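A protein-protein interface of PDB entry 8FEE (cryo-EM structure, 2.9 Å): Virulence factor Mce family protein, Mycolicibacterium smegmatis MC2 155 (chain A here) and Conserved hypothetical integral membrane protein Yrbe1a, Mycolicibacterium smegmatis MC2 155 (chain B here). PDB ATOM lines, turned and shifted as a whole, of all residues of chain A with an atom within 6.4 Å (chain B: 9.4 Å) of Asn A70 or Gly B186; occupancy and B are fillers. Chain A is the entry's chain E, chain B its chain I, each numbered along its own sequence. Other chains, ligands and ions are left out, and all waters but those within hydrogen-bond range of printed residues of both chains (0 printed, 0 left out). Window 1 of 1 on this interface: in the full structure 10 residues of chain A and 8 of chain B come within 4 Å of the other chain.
Val B189 touches Ile A39. Ser B190 touches Ala A40. Leu A44 touches Phe B174. CD1 of Leu A44 touches CB of Ala B185, at 3.7 Å. CD1 of Leu A44 touches CG1 of Val B189 (3.6 Å). Asn A68 touches Ser B190. O of Asn A70 touches CA of Gly B186, at 3.4 Å. Ser B184 touches Arg A72 (CB to NH2, 3.5 Å).
O of Ala A40 lies within hydrogen-bond range of ND2 of Asn A70, at 3.4 Å. The backbone carbonyl oxygen (O) of Val A42 sits at hydrogen-bond distance from the side-chain amide nitrogen (ND2) of Asn A70. The backbone NH (N) of Leu A44 lies within hydrogen-bond range of the side-chain amide oxygen (OD1) of Asn A70 (3.5 Å). O of Leu A44 is in hydrogen-bond range of NH1 of Arg A82 (2.5 Å). OG of Ser A71 is in hydrogen-bond range of O of Asn A68. The backbone NH (N) of Asn A70 is in hydrogen-bond range of the backbone carbonyl oxygen (O) of Val A83, at 2.8 Å.
Hydrophobic or aromatic side chains of chain A within 4 Å of the printed part of chain B: Ile A39, Ala A40 and Leu A44. Along chain A the printed residues that touch a printed residue of chain B span positions 39 to 72. Of the 19 printed residues of chain B, 6 touch a printed residue of chain A. Printed residues of chain B that touch a printed residue of chain A: Phe B174, Ser B184, Ala B185, Gly B186, Val B189 and Ser B190. Hydrophobic or aromatic side chains of chain B that line the printed part of chain A: Phe B174, Ala B185 and Val B189.
Asn A70 touches just one residue of chain B: Gly B186 (3.4 Å). Ala A69 touches none of the printed residues of chain B. No residue of chain B comes within 4 Å of Ser A71. Of the printed residues of chain A, Phe B174 touches Leu A44 (3.9 Å). Of the printed residues of chain B, Ile A39 touches Val B189 (3.4 Å). The nearest residue of chain B that does not touch Asn A70 is Val B189 (4.2 Å). The nearest residue of chain A that does not touch Gly B186 is Leu A44 (4.8 Å).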
ATOM      1  N   ILE A  39     -11.623 -30.339  17.280  1.00  0.00           N
ATOM      2  CA  ILE A  39     -10.966 -31.201  18.256  1.00  0.00           C
ATOM      3  C   ILE A  39      -9.789 -30.498  18.922  1.00  0.00           C
ATOM      4  O   ILE A  39      -9.306 -30.958  19.965  1.00  0.00           O
ATOM      5  CB  ILE A  39     -10.521 -32.513  17.585  1.00  0.00           C
ATOM      6  CG1 ILE A  39     -10.221 -33.597  18.626  1.00  0.00           C
ATOM      7  CG2 ILE A  39      -9.308 -32.277  16.695  1.00  0.00           C
ATOM      8  CD1 ILE A  39     -11.368 -33.872  19.570  1.00  0.00           C
ATOM      9  N   ALA A  40      -9.317 -29.386  18.358  1.00  0.00           N
ATOM     10  CA  ALA A  40      -8.234 -28.639  18.979  1.00  0.00           C
ATOM     11  C   ALA A  40      -8.715 -27.715  20.088  1.00  0.00           C
ATOM     12  O   ALA A  40      -7.925 -27.371  20.972  1.00  0.00           O
ATOM     13  CB  ALA A  40      -7.485 -27.824  17.924  1.00  0.00           C
ATOM     14  N   ASN A  41      -9.984 -27.313  20.066  1.00  0.00           N
ATOM     15  CA  ASN A  41     -10.508 -26.321  20.994  1.00  0.00           C
ATOM     16  C   ASN A  41     -11.334 -26.928  22.120  1.00  0.00           C
ATOM     17  O   ASN A  41     -12.026 -26.191  22.829  1.00  0.00           O
ATOM     18  CB  ASN A  41     -11.342 -25.285  20.239  1.00  0.00           C
ATOM     19  CG  ASN A  41     -10.494 -24.361  19.390  1.00  0.00           C
ATOM     20  OD1 ASN A  41     -10.232 -23.220  19.767  1.00  0.00           O
ATOM     21  ND2 ASN A  41     -10.058 -24.852  18.236  1.00  0.00           N
ATOM     22  N   VAL A  42     -11.285 -28.243  22.303  1.00  0.00           N
ATOM     23  CA  VAL A  42     -12.014 -28.890  23.390  1.00  0.00           C
ATOM     24  C   VAL A  42     -11.118 -28.928  24.625  1.00  0.00           C
ATOM     25  O   VAL A  42      -9.932 -29.273  24.517  1.00  0.00           O
ATOM     26  CB  VAL A  42     -12.500 -30.293  22.980  1.00  0.00           C
ATOM     27  CG1 VAL A  42     -11.361 -31.130  22.426  1.00  0.00           C
ATOM     28  CG2 VAL A  42     -13.164 -31.002  24.148  1.00  0.00           C
ATOM     29  N   PRO A  43     -11.617 -28.544  25.800  1.00  0.00           N
ATOM     30  CA  PRO A  43     -10.788 -28.598  27.016  1.00  0.00           C
ATOM     31  C   PRO A  43     -10.477 -30.039  27.393  1.00  0.00           C
ATOM     32  O   PRO A  43     -11.382 -30.856  27.570  1.00  0.00           O
ATOM     33  CB  PRO A  43     -11.658 -27.908  28.074  1.00  0.00           C
ATOM     34  CG  PRO A  43     -12.687 -27.145  27.298  1.00  0.00           C
ATOM     35  CD  PRO A  43     -12.935 -27.946  26.065  1.00  0.00           C
ATOM     36  N   LEU A  44      -9.184 -30.344  27.524  1.00  0.00           N
ATOM     37  CA  LEU A  44      -8.703 -31.690  27.783  1.00  0.00           C
ATOM     38  C   LEU A  44      -8.349 -31.866  29.255  1.00  0.00           C
ATOM     39  O   LEU A  44      -7.971 -30.904  29.930  1.00  0.00           O
ATOM     40  CB  LEU A  44      -7.469 -31.987  26.927  1.00  0.00           C
ATOM     41  CG  LEU A  44      -7.674 -31.904  25.417  1.00  0.00           C
ATOM     42  CD1 LEU A  44      -6.394 -32.269  24.699  1.00  0.00           C
ATOM     43  CD2 LEU A  44      -8.813 -32.806  24.981  1.00  0.00           C
ATOM     44  N   ASN A  68      -4.816 -21.688  19.807  1.00  0.00           N
ATOM     45  CA  ASN A  68      -5.784 -22.733  20.098  1.00  0.00           C
ATOM     46  C   ASN A  68      -5.946 -22.893  21.602  1.00  0.00           C
ATOM     47  O   ASN A  68      -5.063 -22.540  22.386  1.00  0.00           O
ATOM     48  CB  ASN A  68      -5.358 -24.066  19.478  1.00  0.00           C
ATOM     49  CG  ASN A  68      -5.648 -24.140  17.996  1.00  0.00           C
ATOM     50  OD1 ASN A  68      -6.635 -23.582  17.516  1.00  0.00           O
ATOM     51  ND2 ASN A  68      -4.791 -24.836  17.262  1.00  0.00           N
ATOM     52  N   ALA A  69      -7.096 -23.427  22.002  1.00  0.00           N
ATOM     53  CA  ALA A  69      -7.261 -23.830  23.386  1.00  0.00           C
ATOM     54  C   ALA A  69      -6.334 -25.003  23.699  1.00  0.00           C
ATOM     55  O   ALA A  69      -5.746 -25.621  22.805  1.00  0.00           O
ATOM     56  CB  ALA A  69      -8.715 -24.200  23.669  1.00  0.00           C
ATOM     57  N   ASN A  70      -6.194 -25.293  24.996  1.00  0.00           N
ATOM     58  CA  ASN A  70      -5.262 -26.307  25.497  1.00  0.00           C
ATOM     59  C   ASN A  70      -3.816 -25.959  25.153  1.00  0.00           C
ATOM     60  O   ASN A  70      -2.975 -26.846  24.990  1.00  0.00           O
ATOM     61  CB  ASN A  70      -5.614 -27.711  24.990  1.00  0.00           C
ATOM     62  CG  ASN A  70      -7.093 -28.008  25.081  1.00  0.00           C
ATOM     63  OD1 ASN A  70      -7.772 -27.566  26.007  1.00  0.00           O
ATOM     64  ND2 ASN A  70      -7.605 -28.753  24.111  1.00  0.00           N
ATOM     65  N   SER A  71      -3.516 -24.670  25.035  1.00  0.00           N
ATOM     66  CA  SER A  71      -2.143 -24.210  24.903  1.00  0.00           C
ATOM     67  C   SER A  71      -1.537 -23.967  26.279  1.00  0.00           C
ATOM     68  O   SER A  71      -2.237 -23.881  27.291  1.00  0.00           O
ATOM     69  CB  SER A  71      -2.071 -22.933  24.066  1.00  0.00           C
ATOM     70  OG  SER A  71      -2.053 -23.234  22.683  1.00  0.00           O
ATOM     71  N   ARG A  72      -0.213 -23.851  26.305  1.00  0.00           N
ATOM     72  CA  ARG A  72       0.525 -23.764  27.555  1.00  0.00           C
ATOM     73  C   ARG A  72       0.609 -22.325  28.047  1.00  0.00           C
ATOM     74  O   ARG A  72       0.923 -21.409  27.277  1.00  0.00           O
ATOM     75  CB  ARG A  72       1.927 -24.345  27.377  1.00  0.00           C
ATOM     76  CG  ARG A  72       1.930 -25.823  27.036  1.00  0.00           C
ATOM     77  CD  ARG A  72       3.334 -26.395  27.033  1.00  0.00           C
ATOM     78  NE  ARG A  72       3.318 -27.853  27.057  1.00  0.00           N
ATOM     79  CZ  ARG A  72       4.385 -28.611  27.260  1.00  0.00           C
ATOM     80  NH1 ARG A  72       5.583 -28.082  27.447  1.00  0.00           N
ATOM     81  NH2 ARG A  72       4.249 -29.933  27.277  1.00  0.00           N
ATOM     82  N   ARG A  82      -2.799 -23.893  31.618  1.00  0.00           N
ATOM     83  CA  ARG A  82      -3.475 -24.246  30.379  1.00  0.00           C
ATOM     84  C   ARG A  82      -4.576 -23.231  30.109  1.00  0.00           C
ATOM     85  O   ARG A  82      -5.236 -22.765  31.042  1.00  0.00           O
ATOM     86  CB  ARG A  82      -4.058 -25.662  30.463  1.00  0.00           C
ATOM     87  CG  ARG A  82      -4.672 -26.177  29.179  1.00  0.00           C
ATOM     88  CD  ARG A  82      -5.762 -27.189  29.480  1.00  0.00           C
ATOM     89  NE  ARG A  82      -6.692 -26.687  30.484  1.00  0.00           N
ATOM     90  CZ  ARG A  82      -7.788 -27.323  30.874  1.00  0.00           C
ATOM     91  NH1 ARG A  82      -8.132 -28.488  30.353  1.00  0.00           N
ATOM     92  NH2 ARG A  82      -8.558 -26.772  31.808  1.00  0.00           N
ATOM     93  N   VAL A  83      -4.766 -22.890  28.837  1.00  0.00           N
ATOM     94  CA  VAL A  83      -5.820 -21.968  28.428  1.00  0.00           C
ATOM     95  C   VAL A  83      -7.055 -22.764  28.013  1.00  0.00           C
ATOM     96  O   VAL A  83      -6.973 -23.701  27.209  1.00  0.00           O
ATOM     97  CB  VAL A  83      -5.333 -21.020  27.314  1.00  0.00           C
ATOM     98  CG1 VAL A  83      -4.949 -21.765  26.045  1.00  0.00           C
ATOM     99  CG2 VAL A  83      -6.395 -19.980  27.010  1.00  0.00           C
ATOM    100  N   ARG A  84      -8.193 -22.432  28.621  1.00  0.00           N
ATOM    101  CA  ARG A  84      -9.402 -23.241  28.501  1.00  0.00           C
ATOM    102  C   ARG A  84     -10.260 -22.826  27.307  1.00  0.00           C
ATOM    103  O   ARG A  84     -10.565 -23.649  26.439  1.00  0.00           O
ATOM    104  CB  ARG A  84     -10.204 -23.149  29.802  1.00  0.00           C
ATOM    105  CG  ARG A  84     -11.373 -24.105  29.893  1.00  0.00           C
ATOM    106  CD  ARG A  84     -12.333 -23.671  30.983  1.00  0.00           C
ATOM    107  NE  ARG A  84     -11.644 -23.415  32.241  1.00  0.00           N
ATOM    108  CZ  ARG A  84     -12.241 -22.999  33.349  1.00  0.00           C
ATOM    109  NH1 ARG A  84     -13.544 -22.780  33.393  1.00  0.00           N
ATOM    110  NH2 ARG A  84     -11.511 -22.798  34.444  1.00  0.00           N
ATOM    111  N   LYS A  85     -10.658 -21.556  27.253  1.00  0.00           N
ATOM    112  CA  LYS A  85     -11.539 -21.051  26.210  1.00  0.00           C
ATOM    113  C   LYS A  85     -10.961 -19.771  25.623  1.00  0.00           C
ATOM    114  O   LYS A  85     -10.304 -18.996  26.320  1.00  0.00           O
ATOM    115  CB  LYS A  85     -12.948 -20.794  26.759  1.00  0.00           C
ATOM    116  CG  LYS A  85     -14.039 -20.773  25.707  1.00  0.00           C
ATOM    117  CD  LYS A  85     -15.307 -20.135  26.244  1.00  0.00           C
ATOM    118  CE  LYS A  85     -15.762 -20.797  27.530  1.00  0.00           C
ATOM    119  NZ  LYS A  85     -17.058 -20.240  28.003  1.00  0.00           N
ATOM    120  N   ILE A  86     -11.208 -19.553  24.330  1.00  0.00           N
ATOM    121  CA  ILE A  86     -10.727 -18.358  23.641  1.00  0.00           C
ATOM    122  C   ILE A  86     -11.913 -17.605  23.045  1.00  0.00           C
ATOM    123  O   ILE A  86     -11.833 -17.077  21.930  1.00  0.00           O
ATOM    124  CB  ILE A  86      -9.680 -18.706  22.564  1.00  0.00           C
ATOM    125  CG1 ILE A  86      -8.716 -19.769  23.083  1.00  0.00           C
ATOM    126  CG2 ILE A  86      -8.841 -17.482  22.206  1.00  0.00           C
ATOM    127  CD1 ILE A  86      -7.490 -19.943  22.224  1.00  0.00           C
ATOM    128  N   ALA B  87       9.027 -32.612  18.522  1.00  0.00           N
ATOM    129  CA  ALA B  87       8.029 -33.447  19.171  1.00  0.00           C
ATOM    130  C   ALA B  87       6.668 -32.774  19.277  1.00  0.00           C
ATOM    131  O   ALA B  87       5.753 -33.353  19.871  1.00  0.00           O
ATOM    132  CB  ALA B  87       8.508 -33.857  20.566  1.00  0.00           C
ATOM    133  N   ASP B  88       6.512 -31.568  18.728  1.00  0.00           N
ATOM    134  CA  ASP B  88       5.209 -30.918  18.728  1.00  0.00           C
ATOM    135  C   ASP B  88       4.313 -31.416  17.603  1.00  0.00           C
ATOM    136  O   ASP B  88       3.096 -31.211  17.660  1.00  0.00           O
ATOM    137  CB  ASP B  88       5.377 -29.402  18.623  1.00  0.00           C
ATOM    138  CG  ASP B  88       5.964 -28.794  19.880  1.00  0.00           C
ATOM    139  OD1 ASP B  88       5.549 -29.199  20.986  1.00  0.00           O
ATOM    140  OD2 ASP B  88       6.841 -27.912  19.763  1.00  0.00           O
ATOM    141  N   VAL B  89       4.885 -32.064  16.589  1.00  0.00           N
ATOM    142  CA  VAL B  89       4.122 -32.591  15.466  1.00  0.00           C
ATOM    143  C   VAL B  89       3.793 -34.065  15.662  1.00  0.00           C
ATOM    144  O   VAL B  89       3.363 -34.735  14.715  1.00  0.00           O
ATOM    145  CB  VAL B  89       4.863 -32.368  14.140  1.00  0.00           C
ATOM    146  CG1 VAL B  89       5.048 -30.883  13.883  1.00  0.00           C
ATOM    147  CG2 VAL B  89       6.205 -33.077  14.163  1.00  0.00           C
ATOM    148  N   SER B  90       3.966 -34.578  16.884  1.00  0.00           N
ATOM    149  CA  SER B  90       3.725 -35.987  17.173  1.00  0.00           C
ATOM    150  C   SER B  90       2.303 -36.400  16.839  1.00  0.00           C
ATOM    151  O   SER B  90       2.072 -37.545  16.436  1.00  0.00           O
ATOM    152  CB  SER B  90       4.024 -36.275  18.642  1.00  0.00           C
ATOM    153  OG  SER B  90       3.172 -35.524  19.489  1.00  0.00           O
ATOM    154  N   GLY B  91       1.341 -35.492  17.001  1.00  0.00           N
ATOM    155  CA  GLY B  91      -0.028 -35.806  16.634  1.00  0.00           C
ATOM    156  C   GLY B  91      -0.193 -36.072  15.150  1.00  0.00           C
ATOM    157  O   GLY B  91      -0.916 -36.993  14.758  1.00  0.00           O
ATOM    158  N   ALA B  92       0.503 -35.295  14.311  1.00  0.00           N
ATOM    159  CA  ALA B  92       0.285 -35.344  12.866  1.00  0.00           C
ATOM    160  C   ALA B  92       0.460 -36.756  12.326  1.00  0.00           C
ATOM    161  O   ALA B  92      -0.505 -37.380  11.863  1.00  0.00           O
ATOM    162  CB  ALA B  92       1.233 -34.373  12.162  1.00  0.00           C
ATOM    163  N   PHE B 174      -3.155 -40.721  22.172  1.00  0.00           N
ATOM    164  CA  PHE B 174      -3.179 -39.481  22.942  1.00  0.00           C
ATOM    165  C   PHE B 174      -2.901 -39.748  24.414  1.00  0.00           C
ATOM    166  O   PHE B 174      -2.021 -39.119  25.018  1.00  0.00           O
ATOM    167  CB  PHE B 174      -4.528 -38.781  22.775  1.00  0.00           C
ATOM    168  CG  PHE B 174      -4.859 -37.826  23.887  1.00  0.00           C
ATOM    169  CD1 PHE B 174      -4.245 -36.588  23.959  1.00  0.00           C
ATOM    170  CD2 PHE B 174      -5.796 -38.158  24.853  1.00  0.00           C
ATOM    171  CE1 PHE B 174      -4.550 -35.705  24.978  1.00  0.00           C
ATOM    172  CE2 PHE B 174      -6.102 -37.280  25.873  1.00  0.00           C
ATOM    173  CZ  PHE B 174      -5.479 -36.053  25.936  1.00  0.00           C
ATOM    174  N   VAL B 178       0.584 -38.513  26.303  1.00  0.00           N
ATOM    175  CA  VAL B 178       0.471 -37.446  27.293  1.00  0.00           C
ATOM    176  C   VAL B 178       0.837 -37.955  28.684  1.00  0.00           C
ATOM    177  O   VAL B 178       1.621 -37.325  29.403  1.00  0.00           O
ATOM    178  CB  VAL B 178      -0.940 -36.835  27.264  1.00  0.00           C
ATOM    179  CG1 VAL B 178      -1.169 -35.954  28.481  1.00  0.00           C
ATOM    180  CG2 VAL B 178      -1.135 -36.038  25.987  1.00  0.00           C
ATOM    181  N   VAL B 183       4.390 -35.575  26.439  1.00  0.00           N
ATOM    182  CA  VAL B 183       4.196 -34.687  25.300  1.00  0.00           C
ATOM    183  C   VAL B 183       3.039 -33.758  25.636  1.00  0.00           C
ATOM    184  O   VAL B 183       2.317 -33.978  26.614  1.00  0.00           O
ATOM    185  CB  VAL B 183       3.933 -35.468  24.000  1.00  0.00           C
ATOM    186  CG1 VAL B 183       5.098 -36.394  23.691  1.00  0.00           C
ATOM    187  CG2 VAL B 183       2.634 -36.246  24.100  1.00  0.00           C
ATOM    188  N   SER B 184       2.856 -32.713  24.837  1.00  0.00           N
ATOM    189  CA  SER B 184       1.799 -31.742  25.080  1.00  0.00           C
ATOM    190  C   SER B 184       0.496 -32.220  24.452  1.00  0.00           C
ATOM    191  O   SER B 184       0.479 -32.664  23.300  1.00  0.00           O
ATOM    192  CB  SER B 184       2.196 -30.374  24.530  1.00  0.00           C
ATOM    193  OG  SER B 184       3.184 -30.501  23.523  1.00  0.00           O
ATOM    194  N   ALA B 185      -0.591 -32.137  25.223  1.00  0.00           N
ATOM    195  CA  ALA B 185      -1.903 -32.523  24.714  1.00  0.00           C
ATOM    196  C   ALA B 185      -2.360 -31.591  23.600  1.00  0.00           C
ATOM    197  O   ALA B 185      -2.939 -32.041  22.600  1.00  0.00           O
ATOM    198  CB  ALA B 185      -2.919 -32.539  25.853  1.00  0.00           C
ATOM    199  N   GLY B 186      -2.126 -30.288  23.768  1.00  0.00           N
ATOM    200  CA  GLY B 186      -2.504 -29.334  22.738  1.00  0.00           C
ATOM    201  C   GLY B 186      -1.748 -29.549  21.443  1.00  0.00           C
ATOM    202  O   GLY B 186      -2.315 -29.425  20.356  1.00  0.00           O
ATOM    203  N   ALA B 187      -0.458 -29.875  21.537  1.00  0.00           N
ATOM    204  CA  ALA B 187       0.314 -30.161  20.336  1.00  0.00           C
ATOM    205  C   ALA B 187      -0.117 -31.457  19.670  1.00  0.00           C
ATOM    206  O   ALA B 187       0.221 -31.683  18.505  1.00  0.00           O
ATOM    207  CB  ALA B 187       1.805 -30.215  20.657  1.00  0.00           C
ATOM    208  N   TYR B 188      -0.850 -32.312  20.382  1.00  0.00           N
ATOM    209  CA  TYR B 188      -1.358 -33.549  19.802  1.00  0.00           C
ATOM    210  C   TYR B 188      -2.698 -33.322  19.107  1.00  0.00           C
ATOM    211  O   TYR B 188      -2.839 -33.604  17.914  1.00  0.00           O
ATOM    212  CB  TYR B 188      -1.496 -34.624  20.887  1.00  0.00           C
ATOM    213  CG  TYR B 188      -1.778 -36.003  20.340  1.00  0.00           C
ATOM    214  CD1 TYR B 188      -0.742 -36.839  19.951  1.00  0.00           C
ATOM    215  CD2 TYR B 188      -3.079 -36.464  20.194  1.00  0.00           C
ATOM    216  CE1 TYR B 188      -0.992 -38.096  19.443  1.00  0.00           C
ATOM    217  CE2 TYR B 188      -3.338 -37.719  19.681  1.00  0.00           C
ATOM    218  CZ  TYR B 188      -2.291 -38.531  19.310  1.00  0.00           C
ATOM    219  OH  TYR B 188      -2.544 -39.784  18.805  1.00  0.00           O
ATOM    220  N   VAL B 189      -3.686 -32.810  19.844  1.00  0.00           N
ATOM    221  CA  VAL B 189      -5.029 -32.680  19.284  1.00  0.00           C
ATOM    222  C   VAL B 189      -5.130 -31.587  18.225  1.00  0.00           C
ATOM    223  O   VAL B 189      -6.059 -31.612  17.411  1.00  0.00           O
ATOM    224  CB  VAL B 189      -6.064 -32.434  20.395  1.00  0.00           C
ATOM    225  CG1 VAL B 189      -6.121 -33.627  21.330  1.00  0.00           C
ATOM    226  CG2 VAL B 189      -5.742 -31.161  21.156  1.00  0.00           C
ATOM    227  N   SER B 190      -4.209 -30.625  18.205  1.00  0.00           N
ATOM    228  CA  SER B 190      -4.271 -29.552  17.223  1.00  0.00           C
ATOM    229  C   SER B 190      -3.469 -29.837  15.963  1.00  0.00           C
ATOM    230  O   SER B 190      -3.526 -29.040  15.020  1.00  0.00           O
ATOM    231  CB  SER B 190      -3.788 -28.236  17.838  1.00  0.00           C
ATOM    232  OG  SER B 190      -2.459 -28.358  18.306  1.00  0.00           O
ATOM    233  N   THR B 191      -2.724 -30.939  15.917  1.00  0.00           N
ATOM    234  CA  THR B 191      -1.992 -31.330  14.723  1.00  0.00           C
ATOM    235  C   THR B 191      -2.530 -32.608  14.096  1.00  0.00           C
ATOM    236  O   THR B 191      -1.932 -33.113  13.142  1.00  0.00           O
ATOM    237  CB  THR B 191      -0.504 -31.497  15.041  1.00  0.00           C
ATOM    238  OG1 THR B 191      -0.354 -32.109  16.327  1.00  0.00           O
ATOM    239  CG2 THR B 191       0.192 -30.154  15.041  1.00  0.00           C
ATOM    240  N   LEU B 192      -3.646 -33.138  14.603  1.00  0.00           N
ATOM    241  CA  LEU B 192      -4.241 -34.327  14.003  1.00  0.00           C
ATOM    242  C   LEU B 192      -4.649 -34.075  12.557  1.00  0.00           C
ATOM    243  O   LEU B 192      -4.446 -34.929  11.687  1.00  0.00           O
ATOM    244  CB  LEU B 192      -5.447 -34.781  14.824  1.00  0.00           C
ATOM    245  CG  LEU B 192      -5.170 -35.392  16.196  1.00  0.00           C
ATOM    246  CD1 LEU B 192      -6.472 -35.724  16.902  1.00  0.00           C
ATOM    247  CD2 LEU B 192      -4.300 -36.628  16.066  1.00  0.00           C
ATOM    248  N   THR B 193      -5.216 -32.905  12.279  1.00  0.00           N
ATOM    249  CA  THR B 193      -5.735 -32.579  10.959  1.00  0.00           C
ATOM    250  C   THR B 193      -4.679 -31.996  10.028  1.00  0.00           C
ATOM    251  O   THR B 193      -5.019 -31.577   8.917  1.00  0.00           O
ATOM    252  CB  THR B 193      -6.905 -31.602  11.086  1.00  0.00           C
ATOM    253  OG1 THR B 193      -6.512 -30.491  11.901  1.00  0.00           O
ATOM    254  CG2 THR B 193      -8.100 -32.286  11.724  1.00  0.00           C
